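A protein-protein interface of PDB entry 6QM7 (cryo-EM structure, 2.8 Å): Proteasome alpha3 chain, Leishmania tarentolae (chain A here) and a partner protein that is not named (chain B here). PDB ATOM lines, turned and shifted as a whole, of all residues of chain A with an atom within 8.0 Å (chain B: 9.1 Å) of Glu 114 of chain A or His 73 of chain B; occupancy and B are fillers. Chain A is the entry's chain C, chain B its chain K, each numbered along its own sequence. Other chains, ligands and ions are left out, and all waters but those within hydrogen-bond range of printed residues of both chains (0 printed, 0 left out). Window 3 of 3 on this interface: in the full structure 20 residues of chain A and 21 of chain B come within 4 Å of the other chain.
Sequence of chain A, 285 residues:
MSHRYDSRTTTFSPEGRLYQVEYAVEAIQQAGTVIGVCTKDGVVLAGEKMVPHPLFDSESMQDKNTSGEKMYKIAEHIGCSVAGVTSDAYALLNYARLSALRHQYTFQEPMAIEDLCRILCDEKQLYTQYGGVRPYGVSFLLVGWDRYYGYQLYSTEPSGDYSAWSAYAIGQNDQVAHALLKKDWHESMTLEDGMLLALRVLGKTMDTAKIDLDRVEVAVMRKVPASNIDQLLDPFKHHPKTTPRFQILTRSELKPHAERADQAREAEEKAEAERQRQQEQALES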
ATOM      1  N   ILE A  78      -1.307   7.631  -0.702  1.00  0.00           N
ATOM      2  CA  ILE A  78      -0.651   7.416  -2.028  1.00  0.00           C
ATOM      3  C   ILE A  78      -0.184   5.969  -2.122  1.00  0.00           C
ATOM      4  O   ILE A  78       0.580   5.534  -1.266  1.00  0.00           O
ATOM      5  CB  ILE A  78       0.547   8.354  -2.291  1.00  0.00           C
ATOM      6  CG1 ILE A  78       0.350   9.757  -1.720  1.00  0.00           C
ATOM      7  CG2 ILE A  78       0.874   8.392  -3.778  1.00  0.00           C
ATOM      8  CD1 ILE A  78       1.429  10.728  -2.117  1.00  0.00           C
ATOM      9  N   MET A 111       0.992  15.293   1.266  1.00  0.00           N
ATOM     10  CA  MET A 111       1.478  15.764  -0.048  1.00  0.00           C
ATOM     11  C   MET A 111       0.399  15.520  -1.094  1.00  0.00           C
ATOM     12  O   MET A 111      -0.163  14.407  -1.124  1.00  0.00           O
ATOM     13  CB  MET A 111       2.726  14.988  -0.467  1.00  0.00           C
ATOM     14  CG  MET A 111       3.508  15.690  -1.525  1.00  0.00           C
ATOM     15  SD  MET A 111       5.073  14.888  -1.770  1.00  0.00           S
ATOM     16  CE  MET A 111       6.061  16.277  -2.328  1.00  0.00           C
ATOM     17  N   ALA A 112       0.138  16.507  -1.939  1.00  0.00           N
ATOM     18  CA  ALA A 112      -0.732  16.328  -3.118  1.00  0.00           C
ATOM     19  C   ALA A 112      -0.118  15.267  -4.030  1.00  0.00           C
ATOM     20  O   ALA A 112       1.108  15.175  -4.099  1.00  0.00           O
ATOM     21  CB  ALA A 112      -0.878  17.627  -3.843  1.00  0.00           C
ATOM     22  N   ILE A 113      -0.946  14.503  -4.724  1.00  0.00           N
ATOM     23  CA  ILE A 113      -0.461  13.372  -5.556  1.00  0.00           C
ATOM     24  C   ILE A 113       0.408  13.943  -6.669  1.00  0.00           C
ATOM     25  O   ILE A 113       1.518  13.419  -6.851  1.00  0.00           O
ATOM     26  CB  ILE A 113      -1.621  12.539  -6.111  1.00  0.00           C
ATOM     27  CG1 ILE A 113      -2.600  12.143  -5.010  1.00  0.00           C
ATOM     28  CG2 ILE A 113      -1.086  11.322  -6.832  1.00  0.00           C
ATOM     29  CD1 ILE A 113      -1.929  11.642  -3.766  1.00  0.00           C
ATOM     30  N   GLU A 114      -0.073  14.974  -7.367  1.00  0.00           N
ATOM     31  CA  GLU A 114       0.649  15.577  -8.515  1.00  0.00           C
ATOM     32  C   GLU A 114       2.028  16.048  -8.055  1.00  0.00           C
ATOM     33  O   GLU A 114       2.963  15.932  -8.848  1.00  0.00           O
ATOM     34  CB  GLU A 114      -0.116  16.748  -9.130  1.00  0.00           C
ATOM     35  CG  GLU A 114       0.602  17.344 -10.338  1.00  0.00           C
ATOM     36  CD  GLU A 114      -0.248  18.082 -11.365  1.00  0.00           C
ATOM     37  OE1 GLU A 114       0.252  18.276 -12.502  1.00  0.00           O
ATOM     38  OE2 GLU A 114      -1.396  18.477 -11.032  1.00  0.00           O
ATOM     39  N   ASP A 115       2.128  16.569  -6.830  1.00  0.00           N
ATOM     40  CA  ASP A 115       3.393  17.065  -6.222  1.00  0.00           C
ATOM     41  C   ASP A 115       4.404  15.932  -6.077  1.00  0.00           C
ATOM     42  O   ASP A 115       5.591  16.191  -6.317  1.00  0.00           O
ATOM     43  CB  ASP A 115       3.182  17.665  -4.829  1.00  0.00           C
ATOM     44  CG  ASP A 115       2.834  19.144  -4.815  1.00  0.00           C
ATOM     45  OD1 ASP A 115       2.576  19.704  -5.918  1.00  0.00           O
ATOM     46  OD2 ASP A 115       2.810  19.725  -3.695  1.00  0.00           O
ATOM     47  N   LEU A 116       3.956  14.770  -5.610  1.00  0.00           N
ATOM     48  CA  LEU A 116       4.817  13.583  -5.441  1.00  0.00           C
ATOM     49  C   LEU A 116       5.206  13.091  -6.824  1.00  0.00           C
ATOM     50  O   LEU A 116       6.406  12.908  -7.079  1.00  0.00           O
ATOM     51  CB  LEU A 116       4.088  12.459  -4.712  1.00  0.00           C
ATOM     52  CG  LEU A 116       4.957  11.212  -4.559  1.00  0.00           C
ATOM     53  CD1 LEU A 116       5.764  11.308  -3.275  1.00  0.00           C
ATOM     54  CD2 LEU A 116       4.136   9.940  -4.608  1.00  0.00           C
ATOM     55  N   CYS A 117       4.210  12.853  -7.664  1.00  0.00           N
ATOM     56  CA  CYS A 117       4.414  12.436  -9.070  1.00  0.00           C
ATOM     57  C   CYS A 117       5.484  13.323  -9.722  1.00  0.00           C
ATOM     58  O   CYS A 117       6.386  12.772 -10.368  1.00  0.00           O
ATOM     59  CB  CYS A 117       3.108  12.513  -9.839  1.00  0.00           C
ATOM     60  SG  CYS A 117       3.316  11.939 -11.532  1.00  0.00           S
ATOM     61  N   ARG A 118       5.394  14.636  -9.511  1.00  0.00           N
ATOM     62  CA  ARG A 118       6.322  15.662 -10.048  1.00  0.00           C
ATOM     63  C   ARG A 118       7.717  15.493  -9.438  1.00  0.00           C
ATOM     64  O   ARG A 118       8.686  15.659 -10.182  1.00  0.00           O
ATOM     65  CB  ARG A 118       5.757  17.063  -9.787  1.00  0.00           C
ATOM     66  CG  ARG A 118       6.580  18.199 -10.378  1.00  0.00           C
ATOM     67  CD  ARG A 118       6.026  19.583 -10.084  1.00  0.00           C
ATOM     68  NE  ARG A 118       6.841  20.233  -9.056  1.00  0.00           N
ATOM     69  CZ  ARG A 118       6.531  20.379  -7.761  1.00  0.00           C
ATOM     70  NH1 ARG A 118       7.393  20.990  -6.963  1.00  0.00           N
ATOM     71  NH2 ARG A 118       5.380  19.946  -7.264  1.00  0.00           N
ATOM     72  N   ILE A 119       7.819  15.183  -8.148  1.00  0.00           N
ATOM     73  CA  ILE A 119       9.118  15.042  -7.419  1.00  0.00           C
ATOM     74  C   ILE A 119       9.813  13.754  -7.874  1.00  0.00           C
ATOM     75  O   ILE A 119      11.030  13.781  -8.099  1.00  0.00           O
ATOM     76  CB  ILE A 119       8.909  15.099  -5.886  1.00  0.00           C
ATOM     77  CG1 ILE A 119       9.044  16.536  -5.365  1.00  0.00           C
ATOM     78  CG2 ILE A 119       9.824  14.125  -5.154  1.00  0.00           C
ATOM     79  CD1 ILE A 119       9.424  16.664  -3.892  1.00  0.00           C
ATOM     80  N   LEU A 120       9.050  12.670  -7.935  1.00  0.00           N
ATOM     81  CA  LEU A 120       9.467  11.317  -8.382  1.00  0.00           C
ATOM     82  C   LEU A 120       9.945  11.383  -9.829  1.00  0.00           C
ATOM     83  O   LEU A 120      10.899  10.688 -10.165  1.00  0.00           O
ATOM     84  CB  LEU A 120       8.243  10.408  -8.231  1.00  0.00           C
ATOM     85  CG  LEU A 120       8.382   8.958  -8.668  1.00  0.00           C
ATOM     86  CD1 LEU A 120       9.696   8.352  -8.199  1.00  0.00           C
ATOM     87  CD2 LEU A 120       7.206   8.151  -8.135  1.00  0.00           C
ATOM     88  N   CYS A 121       9.320  12.228 -10.638  1.00  0.00           N
ATOM     89  CA  CYS A 121       9.602  12.370 -12.085  1.00  0.00           C
ATOM     90  C   CYS A 121      10.710  13.388 -12.360  1.00  0.00           C
ATOM     91  O   CYS A 121      11.331  13.282 -13.416  1.00  0.00           O
ATOM     92  CB  CYS A 121       8.325  12.751 -12.806  1.00  0.00           C
ATOM     93  SG  CYS A 121       7.205  11.337 -12.911  1.00  0.00           S
ATOM     94  N   ASP A 122      10.919  14.348 -11.463  1.00  0.00           N
ATOM     95  CA  ASP A 122      12.088  15.265 -11.487  1.00  0.00           C
ATOM     96  C   ASP A 122      13.362  14.441 -11.277  1.00  0.00           C
ATOM     97  O   ASP A 122      14.389  14.795 -11.881  1.00  0.00           O
ATOM     98  CB  ASP A 122      11.963  16.385 -10.443  1.00  0.00           C
ATOM     99  CG  ASP A 122      11.066  17.564 -10.829  1.00  0.00           C
ATOM    100  OD1 ASP A 122      11.096  17.985 -12.017  1.00  0.00           O
ATOM    101  OD2 ASP A 122      10.346  18.070  -9.931  1.00  0.00           O
ATOM    102  N   LEU A 142       0.975   5.939 -10.150  1.00  0.00           N
ATOM    103  CA  LEU A 142       0.645   6.546  -8.839  1.00  0.00           C
ATOM    104  C   LEU A 142      -0.863   6.649  -8.747  1.00  0.00           C
ATOM    105  O   LEU A 142      -1.477   7.131  -9.691  1.00  0.00           O
ATOM    106  CB  LEU A 142       1.244   7.944  -8.705  1.00  0.00           C
ATOM    107  CG  LEU A 142       2.581   7.999  -7.987  1.00  0.00           C
ATOM    108  CD1 LEU A 142       3.572   7.063  -8.658  1.00  0.00           C
ATOM    109  CD2 LEU A 142       3.098   9.424  -7.971  1.00  0.00           C
ATOM    110  N   ASP A 146      -6.156  13.395  -2.604  1.00  0.00           N
ATOM    111  CA  ASP A 146      -5.856  14.663  -1.896  1.00  0.00           C
ATOM    112  C   ASP A 146      -7.116  15.522  -1.935  1.00  0.00           C
ATOM    113  O   ASP A 146      -8.034  15.195  -2.702  1.00  0.00           O
ATOM    114  CB  ASP A 146      -4.627  15.366  -2.481  1.00  0.00           C
ATOM    115  CG  ASP A 146      -4.675  15.634  -3.978  1.00  0.00           C
ATOM    116  OD1 ASP A 146      -5.756  15.491  -4.561  1.00  0.00           O
ATOM    117  OD2 ASP A 146      -3.620  15.974  -4.561  1.00  0.00           O
ATOM    118  N   TYR A 148      -7.374  18.436  -3.058  1.00  0.00           N
ATOM    119  CA  TYR A 148      -7.321  19.348  -4.222  1.00  0.00           C
ATOM    120  C   TYR A 148      -8.142  18.755  -5.362  1.00  0.00           C
ATOM    121  O   TYR A 148      -9.122  19.395  -5.755  1.00  0.00           O
ATOM    122  CB  TYR A 148      -5.870  19.645  -4.602  1.00  0.00           C
ATOM    123  CG  TYR A 148      -5.082  20.305  -3.495  1.00  0.00           C
ATOM    124  CD1 TYR A 148      -5.365  21.603  -3.095  1.00  0.00           C
ATOM    125  CD2 TYR A 148      -4.064  19.634  -2.829  1.00  0.00           C
ATOM    126  CE1 TYR A 148      -4.648  22.224  -2.083  1.00  0.00           C
ATOM    127  CE2 TYR A 148      -3.337  20.240  -1.815  1.00  0.00           C
ATOM    128  CZ  TYR A 148      -3.628  21.543  -1.441  1.00  0.00           C
ATOM    129  OH  TYR A 148      -2.921  22.155  -0.443  1.00  0.00           O
ATOM    130  N   TYR A 149      -7.763  17.587  -5.875  1.00  0.00           N
ATOM    131  CA  TYR A 149      -8.348  17.002  -7.111  1.00  0.00           C
ATOM    132  C   TYR A 149      -9.050  15.675  -6.822  1.00  0.00           C
ATOM    133  O   TYR A 149      -9.596  15.078  -7.763  1.00  0.00           O
ATOM    134  CB  TYR A 149      -7.261  16.854  -8.175  1.00  0.00           C
ATOM    135  CG  TYR A 149      -6.544  18.137  -8.517  1.00  0.00           C
ATOM    136  CD1 TYR A 149      -7.242  19.265  -8.930  1.00  0.00           C
ATOM    137  CD2 TYR A 149      -5.159  18.229  -8.440  1.00  0.00           C
ATOM    138  CE1 TYR A 149      -6.586  20.447  -9.247  1.00  0.00           C
ATOM    139  CE2 TYR A 149      -4.488  19.399  -8.765  1.00  0.00           C
ATOM    140  CZ  TYR A 149      -5.202  20.517  -9.167  1.00  0.00           C
ATOM    141  OH  TYR A 149      -4.539  21.673  -9.481  1.00  0.00           O
ATOM    142  N   GLN A 152      -7.014  10.343  -7.914  1.00  0.00           N
ATOM    143  CA  GLN A 152      -6.102  10.639  -9.032  1.00  0.00           C
ATOM    144  C   GLN A 152      -5.308   9.387  -9.363  1.00  0.00           C
ATOM    145  O   GLN A 152      -5.026   8.613  -8.451  1.00  0.00           O
ATOM    146  CB  GLN A 152      -5.134  11.747  -8.650  1.00  0.00           C
ATOM    147  CG  GLN A 152      -5.803  13.051  -8.283  1.00  0.00           C
ATOM    148  CD  GLN A 152      -4.767  14.005  -7.754  1.00  0.00           C
ATOM    149  OE1 GLN A 152      -3.972  14.579  -8.507  1.00  0.00           O
ATOM    150  NE2 GLN A 152      -4.770  14.166  -6.441  1.00  0.00           N
ATOM    151  N   TYR A 154      -1.900   8.626 -11.925  1.00  0.00           N
ATOM    152  CA  TYR A 154      -0.799   9.186 -12.736  1.00  0.00           C
ATOM    153  C   TYR A 154       0.013   8.040 -13.304  1.00  0.00           C
ATOM    154  O   TYR A 154       0.314   7.109 -12.552  1.00  0.00           O
ATOM    155  CB  TYR A 154       0.067  10.095 -11.879  1.00  0.00           C
ATOM    156  CG  TYR A 154      -0.609  11.405 -11.591  1.00  0.00           C
ATOM    157  CD1 TYR A 154      -0.612  12.426 -12.535  1.00  0.00           C
ATOM    158  CD2 TYR A 154      -1.278  11.617 -10.396  1.00  0.00           C
ATOM    159  CE1 TYR A 154      -1.240  13.636 -12.288  1.00  0.00           C
ATOM    160  CE2 TYR A 154      -1.896  12.828 -10.127  1.00  0.00           C
ATOM    161  CZ  TYR A 154      -1.887  13.833 -11.083  1.00  0.00           C
ATOM    162  OH  TYR A 154      -2.504  15.021 -10.853  1.00  0.00           O
ATOM    163  N   TYR A 162       5.197  12.717 -16.912  1.00  0.00           N
ATOM    164  CA  TYR A 162       4.025  12.065 -16.284  1.00  0.00           C
ATOM    165  C   TYR A 162       2.759  12.667 -16.871  1.00  0.00           C
ATOM    166  O   TYR A 162       2.822  13.757 -17.450  1.00  0.00           O
ATOM    167  CB  TYR A 162       4.013  12.267 -14.768  1.00  0.00           C
ATOM    168  CG  TYR A 162       3.805  13.680 -14.285  1.00  0.00           C
ATOM    169  CD1 TYR A 162       4.884  14.453 -13.887  1.00  0.00           C
ATOM    170  CD2 TYR A 162       2.535  14.232 -14.170  1.00  0.00           C
ATOM    171  CE1 TYR A 162       4.714  15.749 -13.422  1.00  0.00           C
ATOM    172  CE2 TYR A 162       2.349  15.528 -13.711  1.00  0.00           C
ATOM    173  CZ  TYR A 162       3.445  16.290 -13.338  1.00  0.00           C
ATOM    174  OH  TYR A 162       3.301  17.566 -12.867  1.00  0.00           O
ATOM    175  N   SER A 163       1.640  11.994 -16.656  1.00  0.00           N
ATOM    176  CA  SER A 163       0.314  12.392 -17.181  1.00  0.00           C
ATOM    177  C   SER A 163      -0.751  11.888 -16.218  1.00  0.00           C
ATOM    178  O   SER A 163      -0.563  10.821 -15.643  1.00  0.00           O
ATOM    179  CB  SER A 163       0.091  11.865 -18.590  1.00  0.00           C
ATOM    180  OG  SER A 163       1.295  11.372 -19.173  1.00  0.00           O
ATOM    181  N   ALA A 164      -1.817  12.655 -16.037  1.00  0.00           N
ATOM    182  CA  ALA A 164      -3.007  12.236 -15.271  1.00  0.00           C
ATOM    183  C   ALA A 164      -3.887  11.414 -16.206  1.00  0.00           C
ATOM    184  O   ALA A 164      -3.915  11.714 -17.415  1.00  0.00           O
ATOM    185  CB  ALA A 164      -3.725  13.434 -14.721  1.00  0.00           C
ATOM    186  N   ALA B  66       4.269  31.584  -2.647  1.00  0.00           N
ATOM    187  CA  ALA B  66       3.928  31.966  -4.035  1.00  0.00           C
ATOM    188  C   ALA B  66       4.569  30.959  -4.979  1.00  0.00           C
ATOM    189  O   ALA B  66       3.885  30.528  -5.922  1.00  0.00           O
ATOM    190  CB  ALA B  66       4.391  33.365  -4.335  1.00  0.00           C
ATOM    191  N   LEU B  67       5.829  30.595  -4.713  1.00  0.00           N
ATOM    192  CA  LEU B  67       6.573  29.573  -5.492  1.00  0.00           C
ATOM    193  C   LEU B  67       5.806  28.256  -5.431  1.00  0.00           C
ATOM    194  O   LEU B  67       5.632  27.637  -6.491  1.00  0.00           O
ATOM    195  CB  LEU B  67       7.970  29.390  -4.901  1.00  0.00           C
ATOM    196  CG  LEU B  67       8.864  28.392  -5.632  1.00  0.00           C
ATOM    197  CD1 LEU B  67       8.891  28.689  -7.118  1.00  0.00           C
ATOM    198  CD2 LEU B  67      10.269  28.409  -5.058  1.00  0.00           C
ATOM    199  N   ASN B  68       5.386  27.848  -4.230  1.00  0.00           N
ATOM    200  CA  ASN B  68       4.631  26.592  -4.007  1.00  0.00           C
ATOM    201  C   ASN B  68       3.294  26.658  -4.745  1.00  0.00           C
ATOM    202  O   ASN B  68       2.852  25.608  -5.150  1.00  0.00           O
ATOM    203  CB  ASN B  68       4.473  26.268  -2.522  1.00  0.00           C
ATOM    204  CG  ASN B  68       5.787  25.886  -1.870  1.00  0.00           C
ATOM    205  OD1 ASN B  68       6.784  25.693  -2.558  1.00  0.00           O
ATOM    206  ND2 ASN B  68       5.808  25.809  -0.545  1.00  0.00           N
ATOM    207  N   ARG B  69       2.691  27.825  -4.954  1.00  0.00           N
ATOM    208  CA  ARG B  69       1.457  27.932  -5.776  1.00  0.00           C
ATOM    209  C   ARG B  69       1.794  27.751  -7.262  1.00  0.00           C
ATOM    210  O   ARG B  69       1.001  27.103  -7.978  1.00  0.00           O
ATOM    211  CB  ARG B  69       0.760  29.282  -5.613  1.00  0.00           C
ATOM    212  CG  ARG B  69      -0.048  29.426  -4.341  1.00  0.00           C
ATOM    213  CD  ARG B  69      -0.920  30.666  -4.437  1.00  0.00           C
ATOM    214  NE  ARG B  69      -0.188  31.935  -4.397  1.00  0.00           N
ATOM    215  CZ  ARG B  69       0.378  32.479  -3.308  1.00  0.00           C
ATOM    216  NH1 ARG B  69       0.995  33.648  -3.414  1.00  0.00           N
ATOM    217  NH2 ARG B  69       0.352  31.862  -2.132  1.00  0.00           N
ATOM    218  N   MET B  70       2.886  28.362  -7.717  1.00  0.00           N
ATOM    219  CA  MET B  70       3.336  28.324  -9.136  1.00  0.00           C
ATOM    220  C   MET B  70       3.577  26.868  -9.556  1.00  0.00           C
ATOM    221  O   MET B  70       3.162  26.492 -10.678  1.00  0.00           O
ATOM    222  CB  MET B  70       4.623  29.147  -9.327  1.00  0.00           C
ATOM    223  CG  MET B  70       4.451  30.423 -10.137  1.00  0.00           C
ATOM    224  SD  MET B  70       2.884  31.302  -9.858  1.00  0.00           S
ATOM    225  CE  MET B  70       3.350  32.487  -8.595  1.00  0.00           C
ATOM    226  N   ARG B  71       4.221  26.093  -8.678  1.00  0.00           N
ATOM    227  CA  ARG B  71       4.584  24.671  -8.897  1.00  0.00           C
ATOM    228  C   ARG B  71       3.375  23.760  -8.653  1.00  0.00           C
ATOM    229  O   ARG B  71       3.348  22.661  -9.230  1.00  0.00           O
ATOM    230  CB  ARG B  71       5.752  24.301  -7.983  1.00  0.00           C
ATOM    231  CG  ARG B  71       7.064  24.959  -8.384  1.00  0.00           C
ATOM    232  CD  ARG B  71       8.139  24.684  -7.360  1.00  0.00           C
ATOM    233  NE  ARG B  71       9.459  25.008  -7.874  1.00  0.00           N
ATOM    234  CZ  ARG B  71      10.564  25.081  -7.130  1.00  0.00           C
ATOM    235  NH1 ARG B  71      10.521  24.857  -5.822  1.00  0.00           N
ATOM    236  NH2 ARG B  71      11.720  25.390  -7.700  1.00  0.00           N
ATOM    237  N   GLN B  72       2.413  24.194  -7.845  1.00  0.00           N
ATOM    238  CA  GLN B  72       1.173  23.438  -7.536  1.00  0.00           C
ATOM    239  C   GLN B  72       0.008  24.016  -8.354  1.00  0.00           C
ATOM    240  O   GLN B  72      -1.132  23.989  -7.849  1.00  0.00           O
ATOM    241  CB  GLN B  72       0.927  23.461  -6.019  1.00  0.00           C
ATOM    242  CG  GLN B  72       1.997  22.711  -5.220  1.00  0.00           C
ATOM    243  CD  GLN B  72       2.074  23.033  -3.745  1.00  0.00           C
ATOM    244  OE1 GLN B  72       1.093  23.432  -3.122  1.00  0.00           O
ATOM    245  NE2 GLN B  72       3.253  22.846  -3.169  1.00  0.00           N
ATOM    246  N   HIS B  73       0.273  24.515  -9.566  1.00  0.00           N
ATOM    247  CA  HIS B  73      -0.751  24.955 -10.561  1.00  0.00           C
ATOM    248  C   HIS B  73      -1.887  25.736  -9.879  1.00  0.00           C
ATOM    249  O   HIS B  73      -3.072  25.443 -10.149  1.00  0.00           O
ATOM    250  CB  HIS B  73      -1.208  23.741 -11.389  1.00  0.00           C
ATOM    251  CG  HIS B  73      -0.053  23.026 -12.011  1.00  0.00           C
ATOM    252  ND1 HIS B  73       0.282  21.724 -11.681  1.00  0.00           N
ATOM    253  CD2 HIS B  73       0.893  23.455 -12.879  1.00  0.00           C
ATOM    254  CE1 HIS B  73       1.365  21.371 -12.346  1.00  0.00           C
ATOM    255  NE2 HIS B  73       1.757  22.417 -13.093  1.00  0.00           N
ATOM    256  N   GLY B  74      -1.515  26.700  -9.028  1.00  0.00           N
ATOM    257  CA  GLY B  74      -2.411  27.709  -8.432  1.00  0.00           C
ATOM    258  C   GLY B  74      -3.257  27.159  -7.301  1.00  0.00           C
ATOM    259  O   GLY B  74      -4.326  27.744  -7.048  1.00  0.00           O
ATOM    260  N   ARG B  75      -2.801  26.088  -6.642  1.00  0.00           N
ATOM    261  CA  ARG B  75      -3.476  25.489  -5.458  1.00  0.00           C
ATOM    262  C   ARG B  75      -3.110  26.295  -4.209  1.00  0.00           C
ATOM    263  O   ARG B  75      -1.904  26.384  -3.885  1.00  0.00           O
ATOM    264  CB  ARG B  75      -3.077  24.024  -5.248  1.00  0.00           C
ATOM    265  CG  ARG B  75      -3.967  23.028  -5.973  1.00  0.00           C
ATOM    266  CD  ARG B  75      -3.232  21.824  -6.529  1.00  0.00           C
ATOM    267  NE  ARG B  75      -2.141  21.337  -5.697  1.00  0.00           N
ATOM    268  CZ  ARG B  75      -1.116  20.601  -6.127  1.00  0.00           C
ATOM    269  NH1 ARG B  75      -0.991  20.244  -7.400  1.00  0.00           N
ATOM    270  NH2 ARG B  75      -0.193  20.234  -5.259  1.00  0.00           N
ATOM    271  N   HIS B  76      -4.118  26.830  -3.524  1.00  0.00           N
ATOM    272  CA  HIS B  76      -3.939  27.680  -2.324  1.00  0.00           C
ATOM    273  C   HIS B  76      -3.799  26.765  -1.112  1.00  0.00           C
ATOM    274  O   HIS B  76      -4.777  26.076  -0.779  1.00  0.00           O
ATOM    275  CB  HIS B  76      -5.076  28.704  -2.257  1.00  0.00           C
ATOM    276  CG  HIS B  76      -4.869  29.824  -3.226  1.00  0.00           C
ATOM    277  ND1 HIS B  76      -5.319  31.108  -2.989  1.00  0.00           N
ATOM    278  CD2 HIS B  76      -4.206  29.870  -4.404  1.00  0.00           C
ATOM    279  CE1 HIS B  76      -4.967  31.889  -3.994  1.00  0.00           C
ATOM    280  NE2 HIS B  76      -4.280  31.154  -4.872  1.00  0.00           N
ATOM    281  N   VAL B 114     -11.289  24.203  -1.153  1.00  0.00           N
ATOM    282  CA  VAL B 114     -10.350  24.442  -2.287  1.00  0.00           C
ATOM    283  C   VAL B 114     -10.824  23.656  -3.520  1.00  0.00           C
ATOM    284  O   VAL B 114     -10.207  23.824  -4.596  1.00  0.00           O
ATOM    285  CB  VAL B 114      -8.915  24.061  -1.862  1.00  0.00           C
ATOM    286  CG1 VAL B 114      -8.647  22.563  -1.973  1.00  0.00           C
ATOM    287  CG2 VAL B 114      -7.859  24.862  -2.613  1.00  0.00           C
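NH2 of Arg 75 of chain B touches CB of Ala 112 of chain A (3.0 Å). CE1 of His 73 of chain B touches OE1 of Glu 114 of chain A (3.3 Å). CB of Glu 114 of chain A touches NH1 of Arg 75 of chain B (3.998 Å). Arg 118 of chain A touches Arg 71 of chain B. CD1 of Tyr 148 of chain A touches CG of Arg 75 of chain B (3.5 Å). Val 114 of chain B touches Tyr 148 of chain A. Arg 75 of chain B touches Tyr 149 of chain A.
Of the printed residues of chain B, Glu 114 of chain A touches His 73 and Arg 75. Of chain A, only Glu 114 (3.3 Å) comes within 4 Å of His 73 of chain B. Cys 117 of chain A touches none of the printed residues of chain B. Of the printed residues of chain B, Arg 118 of chain A touches Arg 71. Of the printed residues of chain B, Ala 112 of chain A touches Arg 75. Of the printed residues of chain A, Val 114 of chain B touches Tyr 148. Of the printed residues of chain B, Tyr 149 of chain A touches Arg 75. The nearest printed residue of chain B that does not touch Glu 114 of chain A is Arg 71 of chain B (6.1 Å). The nearest residue of chain A that does not touch His 73 of chain B is Tyr 149 of chain A (4.1 Å). The nearest printed residue of chain B that does not touch Ala 112 of chain A is Gln 72 of chain B (6.0 Å).
N of Tyr 149 of chain A lies within hydrogen-bond range of OD1 of Asp 146 of chain A (3.2 Å). The side-chain carboxylate of Glu 114 of chain A sits at hydrogen-bond distance from the side-chain hydroxyl of Tyr 162 of chain A (3.2 Å). OD1 of Asp 115 of chain A lies within salt-bridge range of NH2 of Arg 118 of chain A (3.1 Å). O of Asn 68 of chain B lies close to NE2 of Gln 72 of chain B, 3.4 Å away.
Of the 22 printed residues of chain A, 6 touch a printed residue of chain B. Printed residues of chain A that touch a printed residue of chain B: Ala 112, Glu 114, Asp 115, Arg 118, Tyr 148 and Tyr 149. Along chain A the printed residues that touch a printed residue of chain B span positions 112 to 149. Of the 12 printed residues of chain B, 5 touch a printed residue of chain A. Hydrophobic or aromatic side chains of chain B within 4 Å of the printed part of chain A: His 73 and Val 114. Among the printed residues, 9 pairs touch across the chains.
OD2 of Asp 115 of chain A is in hydrogen-bond range of NE2 of Gln 72 of chain B (3.2 Å). The guanidinium group (NH2) of Arg 75 of chain B is in salt-bridge range of the side-chain carboxylate (OD1) of Asp 115 of chain A, at 2.9 Å.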
